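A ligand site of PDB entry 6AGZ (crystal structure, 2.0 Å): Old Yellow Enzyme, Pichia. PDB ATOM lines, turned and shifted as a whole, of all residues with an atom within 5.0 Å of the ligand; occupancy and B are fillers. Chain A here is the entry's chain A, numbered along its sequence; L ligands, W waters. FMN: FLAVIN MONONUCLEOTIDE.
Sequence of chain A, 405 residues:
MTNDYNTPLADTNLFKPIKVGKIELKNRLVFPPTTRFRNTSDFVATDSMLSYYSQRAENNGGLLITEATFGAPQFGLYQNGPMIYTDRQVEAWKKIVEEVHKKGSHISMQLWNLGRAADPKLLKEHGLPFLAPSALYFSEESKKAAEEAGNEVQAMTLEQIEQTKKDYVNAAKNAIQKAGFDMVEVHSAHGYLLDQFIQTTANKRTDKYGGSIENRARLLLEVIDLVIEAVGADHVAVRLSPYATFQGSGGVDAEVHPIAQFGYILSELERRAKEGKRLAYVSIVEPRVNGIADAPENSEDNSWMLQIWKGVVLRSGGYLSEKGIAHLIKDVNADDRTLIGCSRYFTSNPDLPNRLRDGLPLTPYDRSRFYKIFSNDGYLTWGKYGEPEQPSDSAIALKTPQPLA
Water W1 lies within hydrogen-bond range of O3' of the ligand and NE2 of His 190.
Water W2 lies within hydrogen-bond range of O2P of the ligand (2.9 Å), N of Arg 344 (3.2 Å) and N of Ser 343 (3.4 Å).
The side-chain hydroxyl (OG1) of Thr 34 sits at hydrogen-bond distance from the side-chain hydroxyl (OG) of Ser 343 (2.7 Å).
O of Pro 32 lies within hydrogen-bond range of OG1 of Thr 34.
The guanidinium group of Arg 36 lies within hydrogen-bond range of the backbone carbonyl oxygen of Phe 370.
Merely in contact with the ligand: Pro 32 (3.5 Å), Thr 34 (3.5 Å), Ala 68 (3.2 Å), His 190 (3.95 Å), Gly 317 (3.4 Å), Gly 341 (3.8 Å), Cys 342 (3.3 Å), Arg 367 (3.99 Å), Phe 370 (3.5 Å) and Tyr 371 (3.2 Å).
Hydrophobic or aromatic side chains that line the ligand: Pro 32, Pro 33, Ala 68, His 187, His 190, Phe 370 and Tyr 371.
N of Thr 35 is in hydrogen-bond range of N5 of the ligand, 2.9 Å away.
O4 of the ligand sits at hydrogen-bond distance from OG1 of Thr 35 (2.6 Å).
An oxygen (O1P) of the ligand sits at hydrogen-bond distance from the backbone NH of Gly 318 (2.8 Å).
O2 of the ligand is in hydrogen-bond range of NH1 of Arg 239 (2.8 Å).
The backbone carbonyl oxygen (O) of Pro 33 sits at hydrogen-bond distance from an oxygen (O2') of the ligand (2.8 Å).
O2P of the ligand sits at hydrogen-bond distance from N of Ser 343 (2.9 Å).
The side-chain amide nitrogen (NE2) of Gln 110 lies within hydrogen-bond range of an oxygen (O2) of the ligand (2.9 Å).
An oxygen (O3P) of the ligand sits at hydrogen-bond distance from the backbone NH (N) of Arg 344 (2.9 Å).
An oxygen (O3P) of the ligand lies within salt-bridge range of the guanidinium group (NE) of Arg 344 (2.9 Å).
A ring nitrogen (NE2) of His 187 is in hydrogen-bond range of an oxygen (O2) of the ligand, at 3.4 Å.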
ATOM      1  N   PRO A  32      31.342  13.410  -4.839  1.00  0.00           N
ATOM      2  CA  PRO A  32      31.404  13.944  -3.475  1.00  0.00           C
ATOM      3  C   PRO A  32      30.566  13.100  -2.538  1.00  0.00           C
ATOM      4  O   PRO A  32      29.747  12.271  -2.987  1.00  0.00           O
ATOM      5  CB  PRO A  32      30.825  15.359  -3.625  1.00  0.00           C
ATOM      6  CG  PRO A  32      30.799  15.630  -5.106  1.00  0.00           C
ATOM      7  CD  PRO A  32      30.616  14.297  -5.750  1.00  0.00           C
ATOM      8  N   PRO A  33      30.748  13.241  -1.226  1.00  0.00           N
ATOM      9  CA  PRO A  33      29.910  12.497  -0.275  1.00  0.00           C
ATOM     10  C   PRO A  33      28.438  12.812  -0.486  1.00  0.00           C
ATOM     11  O   PRO A  33      28.041  13.980  -0.517  1.00  0.00           O
ATOM     12  CB  PRO A  33      30.414  12.970   1.088  1.00  0.00           C
ATOM     13  CG  PRO A  33      31.106  14.272   0.819  1.00  0.00           C
ATOM     14  CD  PRO A  33      31.711  14.122  -0.539  1.00  0.00           C
ATOM     15  N   THR A  34      27.635  11.770  -0.637  1.00  0.00           N
ATOM     16  CA  THR A  34      26.208  11.928  -0.925  1.00  0.00           C
ATOM     17  C   THR A  34      25.423  10.950  -0.058  1.00  0.00           C
ATOM     18  O   THR A  34      25.454   9.737  -0.300  1.00  0.00           O
ATOM     19  CB  THR A  34      25.917  11.696  -2.410  1.00  0.00           C
ATOM     20  OG1 THR A  34      26.782  12.519  -3.197  1.00  0.00           O
ATOM     21  CG2 THR A  34      24.473  12.051  -2.725  1.00  0.00           C
ATOM     22  N   THR A  35      24.732  11.477   0.939  1.00  0.00           N
ATOM     23  CA  THR A  35      23.945  10.649   1.851  1.00  0.00           C
ATOM     24  C   THR A  35      22.721  10.100   1.143  1.00  0.00           C
ATOM     25  O   THR A  35      21.981  10.841   0.482  1.00  0.00           O
ATOM     26  CB  THR A  35      23.529  11.477   3.068  1.00  0.00           C
ATOM     27  OG1 THR A  35      24.688  11.806   3.848  1.00  0.00           O
ATOM     28  CG2 THR A  35      22.535  10.707   3.929  1.00  0.00           C
ATOM     29  N   ARG A  36      22.491   8.789   1.277  1.00  0.00           N
ATOM     30  CA  ARG A  36      21.376   8.121   0.630  1.00  0.00           C
ATOM     31  C   ARG A  36      20.527   7.254   1.550  1.00  0.00           C
ATOM     32  O   ARG A  36      19.396   6.922   1.168  1.00  0.00           O
ATOM     33  CB  ARG A  36      21.875   7.250  -0.535  1.00  0.00           C
ATOM     34  CG  ARG A  36      22.696   7.997  -1.576  1.00  0.00           C
ATOM     35  CD  ARG A  36      21.910   9.140  -2.205  1.00  0.00           C
ATOM     36  NE  ARG A  36      20.650   8.687  -2.784  1.00  0.00           N
ATOM     37  CZ  ARG A  36      20.531   8.128  -3.986  1.00  0.00           C
ATOM     38  NH1 ARG A  36      21.608   7.957  -4.744  1.00  0.00           N
ATOM     39  NH2 ARG A  36      19.347   7.755  -4.435  1.00  0.00           N
ATOM     40  N   GLU A  67      29.228   8.366   1.196  1.00  0.00           N
ATOM     41  CA  GLU A  67      28.256   9.063   2.021  1.00  0.00           C
ATOM     42  C   GLU A  67      28.828   9.321   3.409  1.00  0.00           C
ATOM     43  O   GLU A  67      29.634   8.535   3.929  1.00  0.00           O
ATOM     44  CB  GLU A  67      26.987   8.218   2.130  1.00  0.00           C
ATOM     45  CG  GLU A  67      27.290   6.793   2.584  1.00  0.00           C
ATOM     46  CD  GLU A  67      26.268   5.783   2.116  1.00  0.00           C
ATOM     47  OE1 GLU A  67      25.266   5.587   2.823  1.00  0.00           O
ATOM     48  OE2 GLU A  67      26.469   5.197   1.037  1.00  0.00           O
ATOM     49  N   ALA A  68      28.427  10.443   4.004  1.00  0.00           N
ATOM     50  CA  ALA A  68      28.905  10.792   5.329  1.00  0.00           C
ATOM     51  C   ALA A  68      28.600   9.675   6.323  1.00  0.00           C
ATOM     52  O   ALA A  68      27.448   9.256   6.470  1.00  0.00           O
ATOM     53  CB  ALA A  68      28.266  12.108   5.781  1.00  0.00           C
ATOM     54  N   GLN A 110      34.123   9.872   4.118  1.00  0.00           N
ATOM     55  CA  GLN A 110      33.845  11.065   4.905  1.00  0.00           C
ATOM     56  C   GLN A 110      33.267  10.656   6.245  1.00  0.00           C
ATOM     57  O   GLN A 110      32.342   9.835   6.301  1.00  0.00           O
ATOM     58  CB  GLN A 110      32.885  12.004   4.168  1.00  0.00           C
ATOM     59  CG  GLN A 110      32.744  13.356   4.836  1.00  0.00           C
ATOM     60  CD  GLN A 110      31.566  14.163   4.300  1.00  0.00           C
ATOM     61  OE1 GLN A 110      30.454  13.651   4.203  1.00  0.00           O
ATOM     62  NE2 GLN A 110      31.807  15.416   3.958  1.00  0.00           N
ATOM     63  N   TRP A 112      31.201  11.517   9.627  1.00  0.00           N
ATOM     64  CA  TRP A 112      30.087  12.378   9.984  1.00  0.00           C
ATOM     65  C   TRP A 112      29.961  12.483  11.505  1.00  0.00           C
ATOM     66  O   TRP A 112      30.214  11.520  12.227  1.00  0.00           O
ATOM     67  CB  TRP A 112      28.772  11.836   9.404  1.00  0.00           C
ATOM     68  CG  TRP A 112      27.785  12.879   8.990  1.00  0.00           C
ATOM     69  CD1 TRP A 112      27.945  14.236   9.037  1.00  0.00           C
ATOM     70  CD2 TRP A 112      26.478  12.658   8.462  1.00  0.00           C
ATOM     71  NE1 TRP A 112      26.822  14.864   8.569  1.00  0.00           N
ATOM     72  CE2 TRP A 112      25.903  13.913   8.195  1.00  0.00           C
ATOM     73  CE3 TRP A 112      25.736  11.507   8.166  1.00  0.00           C
ATOM     74  CZ2 TRP A 112      24.618  14.056   7.673  1.00  0.00           C
ATOM     75  CZ3 TRP A 112      24.464  11.650   7.640  1.00  0.00           C
ATOM     76  CH2 TRP A 112      23.918  12.915   7.396  1.00  0.00           C
ATOM     77  N   HIS A 187      34.231  15.701   7.873  1.00  0.00           N
ATOM     78  CA  HIS A 187      33.099  16.554   7.540  1.00  0.00           C
ATOM     79  C   HIS A 187      33.024  17.669   8.577  1.00  0.00           C
ATOM     80  O   HIS A 187      32.700  17.423   9.746  1.00  0.00           O
ATOM     81  CB  HIS A 187      31.806  15.731   7.509  1.00  0.00           C
ATOM     82  CG  HIS A 187      30.630  16.450   6.915  1.00  0.00           C
ATOM     83  ND1 HIS A 187      30.596  17.825   6.765  1.00  0.00           N
ATOM     84  CD2 HIS A 187      29.464  15.985   6.436  1.00  0.00           C
ATOM     85  CE1 HIS A 187      29.449  18.165   6.215  1.00  0.00           C
ATOM     86  NE2 HIS A 187      28.741  17.076   6.000  1.00  0.00           N
ATOM     87  N   HIS A 190      28.252  22.410   6.780  1.00  0.00           N
ATOM     88  CA  HIS A 190      26.803  22.244   6.713  1.00  0.00           C
ATOM     89  C   HIS A 190      26.157  22.137   8.096  1.00  0.00           C
ATOM     90  O   HIS A 190      25.179  21.419   8.296  1.00  0.00           O
ATOM     91  CB  HIS A 190      26.439  21.019   5.852  1.00  0.00           C
ATOM     92  CG  HIS A 190      26.849  21.153   4.417  1.00  0.00           C
ATOM     93  ND1 HIS A 190      27.256  20.075   3.662  1.00  0.00           N
ATOM     94  CD2 HIS A 190      26.905  22.229   3.606  1.00  0.00           C
ATOM     95  CE1 HIS A 190      27.546  20.488   2.451  1.00  0.00           C
ATOM     96  NE2 HIS A 190      27.353  21.793   2.379  1.00  0.00           N
ATOM     97  N   ARG A 239      36.239  18.930   4.768  1.00  0.00           N
ATOM     98  CA  ARG A 239      35.308  19.719   3.979  1.00  0.00           C
ATOM     99  C   ARG A 239      34.831  20.916   4.788  1.00  0.00           C
ATOM    100  O   ARG A 239      34.521  20.799   5.978  1.00  0.00           O
ATOM    101  CB  ARG A 239      34.101  18.897   3.510  1.00  0.00           C
ATOM    102  CG  ARG A 239      33.219  19.660   2.544  1.00  0.00           C
ATOM    103  CD  ARG A 239      32.195  18.769   1.874  1.00  0.00           C
ATOM    104  NE  ARG A 239      32.096  19.067   0.453  1.00  0.00           N
ATOM    105  CZ  ARG A 239      31.116  18.620  -0.337  1.00  0.00           C
ATOM    106  NH1 ARG A 239      30.159  17.858   0.150  1.00  0.00           N
ATOM    107  NH2 ARG A 239      31.110  18.943  -1.629  1.00  0.00           N
ATOM    108  N   VAL A 285      32.723  23.983  -1.150  1.00  0.00           N
ATOM    109  CA  VAL A 285      31.433  24.055  -1.834  1.00  0.00           C
ATOM    110  C   VAL A 285      31.322  25.410  -2.511  1.00  0.00           C
ATOM    111  O   VAL A 285      31.498  26.453  -1.859  1.00  0.00           O
ATOM    112  CB  VAL A 285      30.274  23.834  -0.845  1.00  0.00           C
ATOM    113  CG1 VAL A 285      28.959  24.253  -1.489  1.00  0.00           C
ATOM    114  CG2 VAL A 285      30.233  22.374  -0.421  1.00  0.00           C
ATOM    115  N   SER A 316      33.051  21.694  -5.406  1.00  0.00           N
ATOM    116  CA  SER A 316      31.791  21.038  -5.746  1.00  0.00           C
ATOM    117  C   SER A 316      30.638  22.039  -5.729  1.00  0.00           C
ATOM    118  O   SER A 316      30.646  23.012  -4.976  1.00  0.00           O
ATOM    119  CB  SER A 316      31.488  19.884  -4.781  1.00  0.00           C
ATOM    120  OG  SER A 316      32.486  18.879  -4.859  1.00  0.00           O
ATOM    121  N   GLY A 317      29.642  21.766  -6.576  1.00  0.00           N
ATOM    122  CA  GLY A 317      28.393  22.506  -6.570  1.00  0.00           C
ATOM    123  C   GLY A 317      28.064  23.251  -7.851  1.00  0.00           C
ATOM    124  O   GLY A 317      28.738  24.216  -8.210  1.00  0.00           O
ATOM    125  N   GLY A 318      27.013  22.811  -8.549  1.00  0.00           N
ATOM    126  CA  GLY A 318      26.469  23.543  -9.677  1.00  0.00           C
ATOM    127  C   GLY A 318      27.176  23.330 -10.997  1.00  0.00           C
ATOM    128  O   GLY A 318      26.685  23.814 -12.022  1.00  0.00           O
ATOM    129  N   TYR A 319      28.318  22.626 -11.006  1.00  0.00           N
ATOM    130  CA  TYR A 319      29.196  22.619 -12.176  1.00  0.00           C
ATOM    131  C   TYR A 319      28.554  22.002 -13.421  1.00  0.00           C
ATOM    132  O   TYR A 319      29.002  22.293 -14.533  1.00  0.00           O
ATOM    133  CB  TYR A 319      30.490  21.881 -11.851  1.00  0.00           C
ATOM    134  CG  TYR A 319      31.500  22.725 -11.102  1.00  0.00           C
ATOM    135  CD1 TYR A 319      32.060  23.844 -11.699  1.00  0.00           C
ATOM    136  CD2 TYR A 319      31.892  22.401  -9.821  1.00  0.00           C
ATOM    137  CE1 TYR A 319      32.977  24.622 -11.035  1.00  0.00           C
ATOM    138  CE2 TYR A 319      32.822  23.174  -9.139  1.00  0.00           C
ATOM    139  CZ  TYR A 319      33.363  24.277  -9.751  1.00  0.00           C
ATOM    140  OH  TYR A 319      34.280  25.056  -9.087  1.00  0.00           O
ATOM    141  N   GLY A 341      33.897  18.158  -8.280  1.00  0.00           N
ATOM    142  CA  GLY A 341      32.936  17.214  -7.730  1.00  0.00           C
ATOM    143  C   GLY A 341      31.544  17.433  -8.311  1.00  0.00           C
ATOM    144  O   GLY A 341      31.084  18.566  -8.416  1.00  0.00           O
ATOM    145  N   CYS A 342      30.891  16.334  -8.675  1.00  0.00           N
ATOM    146  CA  CYS A 342      29.521  16.352  -9.178  1.00  0.00           C
ATOM    147  C   CYS A 342      28.737  15.283  -8.431  1.00  0.00           C
ATOM    148  O   CYS A 342      28.990  14.085  -8.609  1.00  0.00           O
ATOM    149  CB  CYS A 342      29.486  16.118 -10.691  1.00  0.00           C
ATOM    150  SG  CYS A 342      30.535  17.235 -11.648  1.00  0.00           S
ATOM    151  N   SER A 343      27.777  15.711  -7.604  1.00  0.00           N
ATOM    152  CA  SER A 343      27.051  14.793  -6.725  1.00  0.00           C
ATOM    153  C   SER A 343      25.689  14.405  -7.291  1.00  0.00           C
ATOM    154  O   SER A 343      25.418  13.220  -7.505  1.00  0.00           O
ATOM    155  CB  SER A 343      26.871  15.435  -5.343  1.00  0.00           C
ATOM    156  OG  SER A 343      25.916  14.727  -4.570  1.00  0.00           O
ATOM    157  N   ARG A 344      24.819  15.389  -7.557  1.00  0.00           N
ATOM    158  CA  ARG A 344      23.435  15.087  -7.893  1.00  0.00           C
ATOM    159  C   ARG A 344      23.322  14.326  -9.210  1.00  0.00           C
ATOM    160  O   ARG A 344      22.525  13.385  -9.327  1.00  0.00           O
ATOM    161  CB  ARG A 344      22.613  16.380  -7.930  1.00  0.00           C
ATOM    162  CG  ARG A 344      22.255  16.906  -6.545  1.00  0.00           C
ATOM    163  CD  ARG A 344      21.566  18.256  -6.600  1.00  0.00           C
ATOM    164  NE  ARG A 344      22.501  19.353  -6.840  1.00  0.00           N
ATOM    165  CZ  ARG A 344      22.183  20.636  -6.753  1.00  0.00           C
ATOM    166  NH1 ARG A 344      20.948  21.001  -6.409  1.00  0.00           N
ATOM    167  NH2 ARG A 344      23.091  21.569  -6.987  1.00  0.00           N
ATOM    168  N   ARG A 367      15.323  14.192  -7.171  1.00  0.00           N
ATOM    169  CA  ARG A 367      15.493  14.535  -5.763  1.00  0.00           C
ATOM    170  C   ARG A 367      14.516  13.774  -4.866  1.00  0.00           C
ATOM    171  O   ARG A 367      14.843  13.470  -3.713  1.00  0.00           O
ATOM    172  CB  ARG A 367      15.342  16.045  -5.567  1.00  0.00           C
ATOM    173  CG  ARG A 367      15.076  16.478  -4.129  1.00  0.00           C
ATOM    174  CD  ARG A 367      15.234  17.982  -3.955  1.00  0.00           C
ATOM    175  NE  ARG A 367      16.627  18.395  -4.052  1.00  0.00           N
ATOM    176  CZ  ARG A 367      17.515  18.284  -3.072  1.00  0.00           C
ATOM    177  NH1 ARG A 367      17.146  17.766  -1.896  1.00  0.00           N
ATOM    178  NH2 ARG A 367      18.763  18.693  -3.244  1.00  0.00           N
ATOM    179  N   PHE A 370      16.238  10.839  -3.373  1.00  0.00           N
ATOM    180  CA  PHE A 370      17.541  10.985  -2.737  1.00  0.00           C
ATOM    181  C   PHE A 370      17.597  10.234  -1.414  1.00  0.00           C
ATOM    182  O   PHE A 370      18.562   9.511  -1.136  1.00  0.00           O
ATOM    183  CB  PHE A 370      17.850  12.472  -2.498  1.00  0.00           C
ATOM    184  CG  PHE A 370      18.283  13.218  -3.725  1.00  0.00           C
ATOM    185  CD1 PHE A 370      18.540  12.553  -4.908  1.00  0.00           C
ATOM    186  CD2 PHE A 370      18.446  14.596  -3.689  1.00  0.00           C
ATOM    187  CE1 PHE A 370      18.950  13.252  -6.043  1.00  0.00           C
ATOM    188  CE2 PHE A 370      18.847  15.296  -4.800  1.00  0.00           C
ATOM    189  CZ  PHE A 370      19.097  14.624  -5.982  1.00  0.00           C
ATOM    190  N   TYR A 371      16.562  10.375  -0.583  1.00  0.00           N
ATOM    191  CA  TYR A 371      16.551   9.855   0.777  1.00  0.00           C
ATOM    192  C   TYR A 371      15.484   8.777   0.968  1.00  0.00           C
ATOM    193  O   TYR A 371      14.980   8.604   2.079  1.00  0.00           O
ATOM    194  CB  TYR A 371      16.358  10.984   1.783  1.00  0.00           C
ATOM    195  CG  TYR A 371      17.351  12.117   1.649  1.00  0.00           C
ATOM    196  CD1 TYR A 371      18.684  11.949   1.994  1.00  0.00           C
ATOM    197  CD2 TYR A 371      16.949  13.366   1.180  1.00  0.00           C
ATOM    198  CE1 TYR A 371      19.590  12.986   1.879  1.00  0.00           C
ATOM    199  CE2 TYR A 371      17.853  14.403   1.056  1.00  0.00           C
ATOM    200  CZ  TYR A 371      19.169  14.213   1.416  1.00  0.00           C
ATOM    201  OH  TYR A 371      20.067  15.242   1.294  1.00  0.00           O
HETATM  202  N1  FMN L   1      27.793  16.700   1.350  1.00  0.00           N
HETATM  203  C2  FMN L   1      28.567  16.218   2.392  1.00  0.00           C
HETATM  204  O2  FMN L   1      29.616  16.791   2.699  1.00  0.00           O
HETATM  205  N3  FMN L   1      28.182  15.084   3.087  1.00  0.00           N
HETATM  206  C4  FMN L   1      27.013  14.439   2.733  1.00  0.00           C
HETATM  207  O4  FMN L   1      26.653  13.438   3.352  1.00  0.00           O
HETATM  208  C4A FMN L   1      26.232  14.928   1.692  1.00  0.00           C
HETATM  209  N5  FMN L   1      25.066  14.283   1.347  1.00  0.00           N
HETATM  210  C5A FMN L   1      24.296  14.752   0.316  1.00  0.00           C
HETATM  211  C6  FMN L   1      23.117  14.093  -0.025  1.00  0.00           C
HETATM  212  C7  FMN L   1      22.330  14.561  -1.063  1.00  0.00           C
HETATM  213  C7M FMN L   1      21.066  13.846  -1.429  1.00  0.00           C
HETATM  214  C8  FMN L   1      22.713  15.694  -1.768  1.00  0.00           C
HETATM  215  C8M FMN L   1      21.863  16.204  -2.895  1.00  0.00           C
HETATM  216  C9  FMN L   1      23.884  16.360  -1.426  1.00  0.00           C
HETATM  217  C9A FMN L   1      24.681  15.886  -0.380  1.00  0.00           C
HETATM  218  N10 FMN L   1      25.853  16.538  -0.037  1.00  0.00           N
HETATM  219  C10 FMN L   1      26.631  16.062   0.993  1.00  0.00           C
HETATM  220  C1' FMN L   1      26.281  17.763  -0.801  1.00  0.00           C
HETATM  221  C2' FMN L   1      27.051  17.287  -2.040  1.00  0.00           C
HETATM  222  O2' FMN L   1      28.196  16.579  -1.636  1.00  0.00           O
HETATM  223  C3' FMN L   1      27.443  18.426  -2.977  1.00  0.00           C
HETATM  224  O3' FMN L   1      28.343  19.295  -2.334  1.00  0.00           O
HETATM  225  C4' FMN L   1      26.216  19.197  -3.456  1.00  0.00           C
HETATM  226  O4' FMN L   1      25.229  18.289  -3.886  1.00  0.00           O
HETATM  227  C5' FMN L   1      26.550  20.132  -4.614  1.00  0.00           C
HETATM  228  O5' FMN L   1      27.155  19.392  -5.660  1.00  0.00           O
HETATM  229  P   FMN L   1      26.348  19.130  -7.025  1.00  0.00           P
HETATM  230  O1P FMN L   1      25.844  20.448  -7.563  1.00  0.00           O
HETATM  231  O2P FMN L   1      27.274  18.487  -8.038  1.00  0.00           O
HETATM  232  O3P FMN L   1      25.189  18.199  -6.744  1.00  0.00           O
HETATM  233  O   HOH W   1      27.107  20.886  -0.585  1.00  0.00           O
HETATM  234  O   HOH W   2      25.907  17.010 -10.118  1.00  0.00           O
HETATM  235  O   HOH W   3      29.022  20.090  -8.960  1.00  0.00           O
